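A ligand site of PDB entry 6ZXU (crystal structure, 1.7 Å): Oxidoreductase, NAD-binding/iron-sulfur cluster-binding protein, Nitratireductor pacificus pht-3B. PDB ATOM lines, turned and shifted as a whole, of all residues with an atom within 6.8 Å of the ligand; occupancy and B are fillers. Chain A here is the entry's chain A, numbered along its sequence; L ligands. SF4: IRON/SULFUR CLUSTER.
The side-chain sulfur (SG) of Cys 595 is bound to an iron atom (FE3) of the ligand, 2.2 Å away. The side-chain sulfur (SG) of Cys 542 is bound to an iron atom (FE2) of the ligand. The backbone NH (N) of Cys 545 sits close to a sulfur (S4) of the ligand. SG of Cys 545 binds FE1 of the ligand, at 2.3 Å. An iron atom (FE4) of the ligand is bound by the side-chain sulfur (SG) of Cys 539.
The guanidinium group (NE) of Arg 500 lies within hydrogen-bond range of the backbone carbonyl oxygen (O) of Cys 542, 3.1 Å away. The backbone NH (N) of Ile 501 sits close to the side-chain hydroxyl (OG) of Ser 499 (3.4 Å). O of Cys 539 sits at hydrogen-bond distance from NH2 of Arg 500 (3.0 Å). The side-chain sulfur (SG) of Cys 542 lies close to the backbone NH (N) of Lys 544 (3.7 Å). The side-chain sulfur (SG) of Cys 595 sits close to the backbone NH (N) of Trp 597, at 3.6 Å.
Ser 499 touches the ligand (CB to S2, 3.9 Å). CB of Arg 500 touches S3 of the ligand, at 3.6 Å. Ile 501 touches the ligand (CG1 to S2, 3.7 Å). Leu 506 touches the ligand (CD1 to S2, 3.96 Å). Phe 538 touches the ligand. Lys 544 touches the ligand (CB to S4, 3.98 Å). CD of Pro 596 touches S4 of the ligand (3.5 Å). CD1 of Trp 597 touches S1 of the ligand, at 3.7 Å. Hydrophobic or aromatic side chains that line the ligand: Ile 501, Leu 506, Phe 538, Pro 596 and Trp 597. 12 residues have an atom within 4 Å of the ligand: Ser 499, Arg 500, Ile 501, Leu 506, Phe 538, Cys 539, Cys 542, Lys 544, Cys 545, Cys 595, Pro 596 and Trp 597.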
ATOM      1  N   SER A 499      -8.668 -21.635 -18.324  1.00  0.00           N
ATOM      2  CA  SER A 499      -7.640 -20.682 -17.974  1.00  0.00           C
ATOM      3  C   SER A 499      -6.245 -21.344 -18.061  1.00  0.00           C
ATOM      4  O   SER A 499      -6.102 -22.553 -18.103  1.00  0.00           O
ATOM      5  CB  SER A 499      -7.846 -20.095 -16.593  1.00  0.00           C
ATOM      6  OG  SER A 499      -7.404 -20.998 -15.593  1.00  0.00           O
ATOM      7  N   ARG A 500      -5.229 -20.496 -18.042  1.00  0.00           N
ATOM      8  CA  ARG A 500      -3.842 -21.010 -18.061  1.00  0.00           C
ATOM      9  C   ARG A 500      -3.536 -21.866 -16.853  1.00  0.00           C
ATOM     10  O   ARG A 500      -2.800 -22.842 -16.934  1.00  0.00           O
ATOM     11  CB  ARG A 500      -2.866 -19.847 -18.223  1.00  0.00           C
ATOM     12  CG  ARG A 500      -1.383 -20.287 -18.161  1.00  0.00           C
ATOM     13  CD  ARG A 500      -0.377 -19.131 -18.375  1.00  0.00           C
ATOM     14  NE  ARG A 500      -0.556 -18.519 -19.649  1.00  0.00           N
ATOM     15  CZ  ARG A 500      -0.164 -18.979 -20.816  1.00  0.00           C
ATOM     16  NH1 ARG A 500       0.571 -20.103 -20.869  1.00  0.00           N
ATOM     17  NH2 ARG A 500      -0.418 -18.291 -21.888  1.00  0.00           N
ATOM     18  N   ILE A 501      -4.090 -21.580 -15.707  1.00  0.00           N
ATOM     19  CA  ILE A 501      -3.879 -22.445 -14.523  1.00  0.00           C
ATOM     20  C   ILE A 501      -3.972 -23.904 -14.831  1.00  0.00           C
ATOM     21  O   ILE A 501      -3.121 -24.658 -14.458  1.00  0.00           O
ATOM     22  CB  ILE A 501      -4.785 -22.022 -13.365  1.00  0.00           C
ATOM     23  CG1 ILE A 501      -4.457 -20.609 -12.954  1.00  0.00           C
ATOM     24  CG2 ILE A 501      -4.622 -22.930 -12.202  1.00  0.00           C
ATOM     25  CD1 ILE A 501      -5.323 -19.983 -11.797  1.00  0.00           C
ATOM     26  N   GLY A 502      -5.003 -24.328 -15.548  1.00  0.00           N
ATOM     27  CA  GLY A 502      -4.967 -25.603 -16.184  1.00  0.00           C
ATOM     28  C   GLY A 502      -6.146 -26.423 -15.834  1.00  0.00           C
ATOM     29  O   GLY A 502      -7.095 -26.560 -16.657  1.00  0.00           O
ATOM     30  N   LEU A 506     -11.957 -20.315 -14.669  1.00  0.00           N
ATOM     31  CA  LEU A 506     -11.936 -18.989 -14.160  1.00  0.00           C
ATOM     32  C   LEU A 506     -13.269 -18.270 -14.466  1.00  0.00           C
ATOM     33  O   LEU A 506     -13.756 -18.254 -15.565  1.00  0.00           O
ATOM     34  CB  LEU A 506     -10.737 -18.248 -14.743  1.00  0.00           C
ATOM     35  CG  LEU A 506     -10.281 -16.910 -14.196  1.00  0.00           C
ATOM     36  CD1 LEU A 506      -8.844 -16.737 -14.464  1.00  0.00           C
ATOM     37  CD2 LEU A 506     -11.070 -15.720 -14.745  1.00  0.00           C
ATOM     38  N   PRO A 512     -10.333 -17.179 -10.290  1.00  0.00           N
ATOM     39  CA  PRO A 512     -10.154 -18.611 -10.100  1.00  0.00           C
ATOM     40  C   PRO A 512     -10.311 -19.050  -8.613  1.00  0.00           C
ATOM     41  O   PRO A 512      -9.975 -20.178  -8.278  1.00  0.00           O
ATOM     42  CB  PRO A 512      -8.702 -18.840 -10.508  1.00  0.00           C
ATOM     43  CG  PRO A 512      -8.051 -17.593 -10.078  1.00  0.00           C
ATOM     44  CD  PRO A 512      -9.068 -16.454 -10.240  1.00  0.00           C
ATOM     45  N   LEU A 535     -11.420 -14.489 -22.067  1.00  0.00           N
ATOM     46  CA  LEU A 535     -10.307 -15.026 -21.262  1.00  0.00           C
ATOM     47  C   LEU A 535      -9.244 -15.649 -22.119  1.00  0.00           C
ATOM     48  O   LEU A 535      -8.078 -15.601 -21.744  1.00  0.00           O
ATOM     49  CB  LEU A 535     -10.774 -15.994 -20.185  1.00  0.00           C
ATOM     50  CG  LEU A 535      -9.721 -16.390 -19.173  1.00  0.00           C
ATOM     51  CD1 LEU A 535      -9.310 -15.202 -18.287  1.00  0.00           C
ATOM     52  CD2 LEU A 535     -10.209 -17.520 -18.341  1.00  0.00           C
ATOM     53  N   PHE A 538      -6.939 -12.990 -22.954  1.00  0.00           N
ATOM     54  CA  PHE A 538      -6.303 -12.470 -21.779  1.00  0.00           C
ATOM     55  C   PHE A 538      -5.199 -13.422 -21.298  1.00  0.00           C
ATOM     56  O   PHE A 538      -4.037 -12.988 -21.095  1.00  0.00           O
ATOM     57  CB  PHE A 538      -7.299 -12.295 -20.654  1.00  0.00           C
ATOM     58  CG  PHE A 538      -6.799 -11.401 -19.525  1.00  0.00           C
ATOM     59  CD1 PHE A 538      -5.980 -11.886 -18.613  1.00  0.00           C
ATOM     60  CD2 PHE A 538      -7.288 -10.114 -19.369  1.00  0.00           C
ATOM     61  CE1 PHE A 538      -5.522 -11.100 -17.570  1.00  0.00           C
ATOM     62  CE2 PHE A 538      -6.895  -9.315 -18.315  1.00  0.00           C
ATOM     63  CZ  PHE A 538      -6.014  -9.807 -17.430  1.00  0.00           C
ATOM     64  N   CYS A 539      -5.550 -14.680 -20.998  1.00  0.00           N
ATOM     65  CA  CYS A 539      -4.553 -15.649 -20.524  1.00  0.00           C
ATOM     66  C   CYS A 539      -3.460 -15.811 -21.560  1.00  0.00           C
ATOM     67  O   CYS A 539      -2.323 -16.044 -21.268  1.00  0.00           O
ATOM     68  CB  CYS A 539      -5.140 -17.012 -20.261  1.00  0.00           C
ATOM     69  SG  CYS A 539      -5.978 -17.118 -18.736  1.00  0.00           S
ATOM     70  N   ASN A 540      -3.748 -15.607 -22.827  1.00  0.00           N
ATOM     71  CA  ASN A 540      -2.692 -15.725 -23.781  1.00  0.00           C
ATOM     72  C   ASN A 540      -1.562 -14.694 -23.665  1.00  0.00           C
ATOM     73  O   ASN A 540      -0.469 -14.850 -24.162  1.00  0.00           O
ATOM     74  CB  ASN A 540      -3.218 -15.580 -25.155  1.00  0.00           C
ATOM     75  CG  ASN A 540      -2.587 -16.557 -26.014  1.00  0.00           C
ATOM     76  OD1 ASN A 540      -2.809 -17.821 -25.828  1.00  0.00           O
ATOM     77  ND2 ASN A 540      -1.682 -16.075 -26.868  1.00  0.00           N
ATOM     78  N   GLN A 541      -1.863 -13.591 -23.018  1.00  0.00           N
ATOM     79  CA  GLN A 541      -0.939 -12.480 -22.870  1.00  0.00           C
ATOM     80  C   GLN A 541      -0.403 -12.356 -21.451  1.00  0.00           C
ATOM     81  O   GLN A 541       0.322 -11.434 -21.185  1.00  0.00           O
ATOM     82  CB  GLN A 541      -1.655 -11.132 -23.172  1.00  0.00           C
ATOM     83  CG  GLN A 541      -2.252 -10.959 -24.516  1.00  0.00           C
ATOM     84  CD  GLN A 541      -2.925  -9.622 -24.666  1.00  0.00           C
ATOM     85  OE1 GLN A 541      -2.296  -8.580 -24.631  1.00  0.00           O
ATOM     86  NE2 GLN A 541      -4.180  -9.648 -24.833  1.00  0.00           N
ATOM     87  N   CYS A 542      -0.828 -13.188 -20.536  1.00  0.00           N
ATOM     88  CA  CYS A 542      -0.461 -13.151 -19.166  1.00  0.00           C
ATOM     89  C   CYS A 542       0.314 -14.447 -18.810  1.00  0.00           C
ATOM     90  O   CYS A 542       0.117 -15.493 -19.424  1.00  0.00           O
ATOM     91  CB  CYS A 542      -1.715 -13.041 -18.305  1.00  0.00           C
ATOM     92  SG  CYS A 542      -1.579 -12.883 -16.516  1.00  0.00           S
ATOM     93  N   ARG A 543       1.174 -14.378 -17.808  1.00  0.00           N
ATOM     94  CA  ARG A 543       1.886 -15.553 -17.283  1.00  0.00           C
ATOM     95  C   ARG A 543       2.044 -15.514 -15.811  1.00  0.00           C
ATOM     96  O   ARG A 543       2.935 -16.184 -15.272  1.00  0.00           O
ATOM     97  CB  ARG A 543       3.286 -15.674 -17.872  1.00  0.00           C
ATOM     98  CG  ARG A 543       3.392 -15.734 -19.374  1.00  0.00           C
ATOM     99  CD  ARG A 543       2.884 -17.033 -19.902  1.00  0.00           C
ATOM    100  NE  ARG A 543       3.046 -17.158 -21.366  1.00  0.00           N
ATOM    101  CZ  ARG A 543       2.327 -16.520 -22.303  1.00  0.00           C
ATOM    102  NH1 ARG A 543       1.367 -15.665 -21.965  1.00  0.00           N
ATOM    103  NH2 ARG A 543       2.576 -16.734 -23.572  1.00  0.00           N
ATOM    104  N   LYS A 544       1.214 -14.785 -15.099  1.00  0.00           N
ATOM    105  CA  LYS A 544       1.473 -14.554 -13.669  1.00  0.00           C
ATOM    106  C   LYS A 544       1.386 -15.850 -12.833  1.00  0.00           C
ATOM    107  O   LYS A 544       2.215 -16.094 -11.965  1.00  0.00           O
ATOM    108  CB  LYS A 544       0.604 -13.433 -13.170  1.00  0.00           C
ATOM    109  CG  LYS A 544       0.885 -13.034 -11.702  1.00  0.00           C
ATOM    110  CD  LYS A 544       0.408 -11.645 -11.418  1.00  0.00           C
ATOM    111  CE  LYS A 544       0.659 -11.304  -9.955  1.00  0.00           C
ATOM    112  NZ  LYS A 544       0.566  -9.830  -9.733  1.00  0.00           N
ATOM    113  N   CYS A 545       0.327 -16.635 -13.008  1.00  0.00           N
ATOM    114  CA  CYS A 545       0.171 -17.882 -12.322  1.00  0.00           C
ATOM    115  C   CYS A 545       1.374 -18.782 -12.602  1.00  0.00           C
ATOM    116  O   CYS A 545       1.854 -19.416 -11.677  1.00  0.00           O
ATOM    117  CB  CYS A 545      -1.132 -18.581 -12.740  1.00  0.00           C
ATOM    118  SG  CYS A 545      -1.322 -18.830 -14.575  1.00  0.00           S
ATOM    119  N   ALA A 546       1.759 -18.921 -13.860  1.00  0.00           N
ATOM    120  CA  ALA A 546       2.894 -19.741 -14.203  1.00  0.00           C
ATOM    121  C   ALA A 546       4.190 -19.306 -13.481  1.00  0.00           C
ATOM    122  O   ALA A 546       4.965 -20.140 -12.993  1.00  0.00           O
ATOM    123  CB  ALA A 546       3.068 -19.731 -15.722  1.00  0.00           C
ATOM    124  N   ILE A 554       2.660 -24.976 -13.949  1.00  0.00           N
ATOM    125  CA  ILE A 554       1.728 -24.321 -14.904  1.00  0.00           C
ATOM    126  C   ILE A 554       2.476 -24.043 -16.198  1.00  0.00           C
ATOM    127  O   ILE A 554       3.579 -23.504 -16.181  1.00  0.00           O
ATOM    128  CB  ILE A 554       1.086 -23.060 -14.251  1.00  0.00           C
ATOM    129  CG1 ILE A 554       0.251 -23.509 -13.061  1.00  0.00           C
ATOM    130  CG2 ILE A 554       0.322 -22.250 -15.268  1.00  0.00           C
ATOM    131  CD1 ILE A 554      -0.330 -22.402 -12.254  1.00  0.00           C
ATOM    132  N   TRP A 568      -4.860 -25.673 -21.514  1.00  0.00           N
ATOM    133  CA  TRP A 568      -3.495 -25.441 -21.050  1.00  0.00           C
ATOM    134  C   TRP A 568      -3.198 -26.544 -20.016  1.00  0.00           C
ATOM    135  O   TRP A 568      -3.729 -26.503 -18.916  1.00  0.00           O
ATOM    136  CB  TRP A 568      -3.345 -24.084 -20.351  1.00  0.00           C
ATOM    137  CG  TRP A 568      -3.101 -22.876 -21.271  1.00  0.00           C
ATOM    138  CD1 TRP A 568      -1.945 -22.593 -21.929  1.00  0.00           C
ATOM    139  CD2 TRP A 568      -4.013 -21.853 -21.606  1.00  0.00           C
ATOM    140  NE1 TRP A 568      -2.083 -21.474 -22.670  1.00  0.00           N
ATOM    141  CE2 TRP A 568      -3.358 -20.991 -22.495  1.00  0.00           C
ATOM    142  CE3 TRP A 568      -5.337 -21.609 -21.303  1.00  0.00           C
ATOM    143  CZ2 TRP A 568      -3.961 -19.831 -23.020  1.00  0.00           C
ATOM    144  CZ3 TRP A 568      -5.923 -20.478 -21.787  1.00  0.00           C
ATOM    145  CH2 TRP A 568      -5.256 -19.618 -22.691  1.00  0.00           C
ATOM    146  N   CYS A 591      -1.682 -20.332  -7.113  1.00  0.00           N
ATOM    147  CA  CYS A 591      -2.092 -19.925  -8.459  1.00  0.00           C
ATOM    148  C   CYS A 591      -3.398 -19.194  -8.398  1.00  0.00           C
ATOM    149  O   CYS A 591      -3.622 -18.215  -9.155  1.00  0.00           O
ATOM    150  CB  CYS A 591      -2.124 -21.175  -9.357  1.00  0.00           C
ATOM    151  SG  CYS A 591      -2.988 -22.592  -8.643  1.00  0.00           S
ATOM    152  N   MET A 594      -2.516 -15.498  -7.113  1.00  0.00           N
ATOM    153  CA  MET A 594      -1.715 -14.590  -7.890  1.00  0.00           C
ATOM    154  C   MET A 594      -2.416 -14.042  -9.151  1.00  0.00           C
ATOM    155  O   MET A 594      -2.013 -13.030  -9.756  1.00  0.00           O
ATOM    156  CB  MET A 594      -0.366 -15.248  -8.207  1.00  0.00           C
ATOM    157  CG  MET A 594       0.471 -15.589  -6.988  1.00  0.00           C
ATOM    158  SD  MET A 594       1.008 -14.121  -6.093  1.00  0.00           S
ATOM    159  CE  MET A 594      -0.098 -14.217  -4.951  1.00  0.00           C
ATOM    160  N   CYS A 595      -3.504 -14.652  -9.547  1.00  0.00           N
ATOM    161  CA  CYS A 595      -4.202 -14.281 -10.722  1.00  0.00           C
ATOM    162  C   CYS A 595      -4.732 -12.839 -10.679  1.00  0.00           C
ATOM    163  O   CYS A 595      -5.373 -12.476  -9.739  1.00  0.00           O
ATOM    164  CB  CYS A 595      -5.343 -15.288 -11.004  1.00  0.00           C
ATOM    165  SG  CYS A 595      -6.150 -15.027 -12.602  1.00  0.00           S
ATOM    166  N   PRO A 596      -4.504 -12.039 -11.749  1.00  0.00           N
ATOM    167  CA  PRO A 596      -5.090 -10.706 -11.791  1.00  0.00           C
ATOM    168  C   PRO A 596      -6.598 -10.656 -11.590  1.00  0.00           C
ATOM    169  O   PRO A 596      -7.107  -9.679 -11.045  1.00  0.00           O
ATOM    170  CB  PRO A 596      -4.735 -10.186 -13.180  1.00  0.00           C
ATOM    171  CG  PRO A 596      -3.530 -10.934 -13.526  1.00  0.00           C
ATOM    172  CD  PRO A 596      -3.713 -12.310 -12.938  1.00  0.00           C
ATOM    173  N   TRP A 597      -7.317 -11.670 -11.996  1.00  0.00           N
ATOM    174  CA  TRP A 597      -8.779 -11.730 -11.810  1.00  0.00           C
ATOM    175  C   TRP A 597      -9.223 -11.995 -10.377  1.00  0.00           C
ATOM    176  O   TRP A 597     -10.414 -11.895 -10.069  1.00  0.00           O
ATOM    177  CB  TRP A 597      -9.394 -12.786 -12.706  1.00  0.00           C
ATOM    178  CG  TRP A 597      -9.257 -12.485 -14.196  1.00  0.00           C
ATOM    179  CD1 TRP A 597      -8.220 -12.770 -14.955  1.00  0.00           C
ATOM    180  CD2 TRP A 597     -10.253 -11.889 -15.042  1.00  0.00           C
ATOM    181  NE1 TRP A 597      -8.472 -12.424 -16.260  1.00  0.00           N
ATOM    182  CE2 TRP A 597      -9.709 -11.839 -16.347  1.00  0.00           C
ATOM    183  CE3 TRP A 597     -11.569 -11.421 -14.859  1.00  0.00           C
ATOM    184  CZ2 TRP A 597     -10.402 -11.394 -17.423  1.00  0.00           C
ATOM    185  CZ3 TRP A 597     -12.252 -10.932 -15.932  1.00  0.00           C
ATOM    186  CH2 TRP A 597     -11.655 -10.879 -17.207  1.00  0.00           C
ATOM    187  N   ASN A 598      -8.289 -12.349  -9.516  1.00  0.00           N
ATOM    188  CA  ASN A 598      -8.542 -12.438  -8.116  1.00  0.00           C
ATOM    189  C   ASN A 598      -8.461 -11.044  -7.528  1.00  0.00           C
ATOM    190  O   ASN A 598      -7.362 -10.529  -7.293  1.00  0.00           O
ATOM    191  CB  ASN A 598      -7.571 -13.462  -7.450  1.00  0.00           C
ATOM    192  CG  ASN A 598      -7.709 -13.487  -5.888  1.00  0.00           C
ATOM    193  OD1 ASN A 598      -8.803 -13.394  -5.347  1.00  0.00           O
ATOM    194  ND2 ASN A 598      -6.582 -13.430  -5.211  1.00  0.00           N
ATOM    195  N   ILE A 623      -2.622  -6.431 -17.251  1.00  0.00           N
ATOM    196  CA  ILE A 623      -1.692  -7.506 -16.883  1.00  0.00           C
ATOM    197  C   ILE A 623      -0.402  -6.927 -16.297  1.00  0.00           C
ATOM    198  O   ILE A 623       0.065  -7.358 -15.236  1.00  0.00           O
ATOM    199  CB  ILE A 623      -1.446  -8.410 -18.134  1.00  0.00           C
ATOM    200  CG1 ILE A 623      -2.667  -9.233 -18.422  1.00  0.00           C
ATOM    201  CG2 ILE A 623      -0.261  -9.290 -17.943  1.00  0.00           C
ATOM    202  CD1 ILE A 623      -2.712  -9.704 -19.861  1.00  0.00           C
HETATM  203 FE1  SF4 L   1      -2.883 -17.325 -15.196  1.00  0.00          FE
HETATM  204 FE2  SF4 L   1      -2.967 -14.621 -15.918  1.00  0.00          FE
HETATM  205 FE3  SF4 L   1      -4.938 -15.647 -14.382  1.00  0.00          FE
HETATM  206 FE4  SF4 L   1      -4.808 -16.443 -16.983  1.00  0.00          FE
HETATM  207  S1  SF4 L   1      -5.146 -14.359 -16.134  1.00  0.00           S
HETATM  208  S2  SF4 L   1      -5.089 -17.732 -15.236  1.00  0.00           S
HETATM  209  S3  SF4 L   1      -2.570 -16.444 -17.171  1.00  0.00           S
HETATM  210  S4  SF4 L   1      -2.731 -15.463 -13.945  1.00  0.00           S
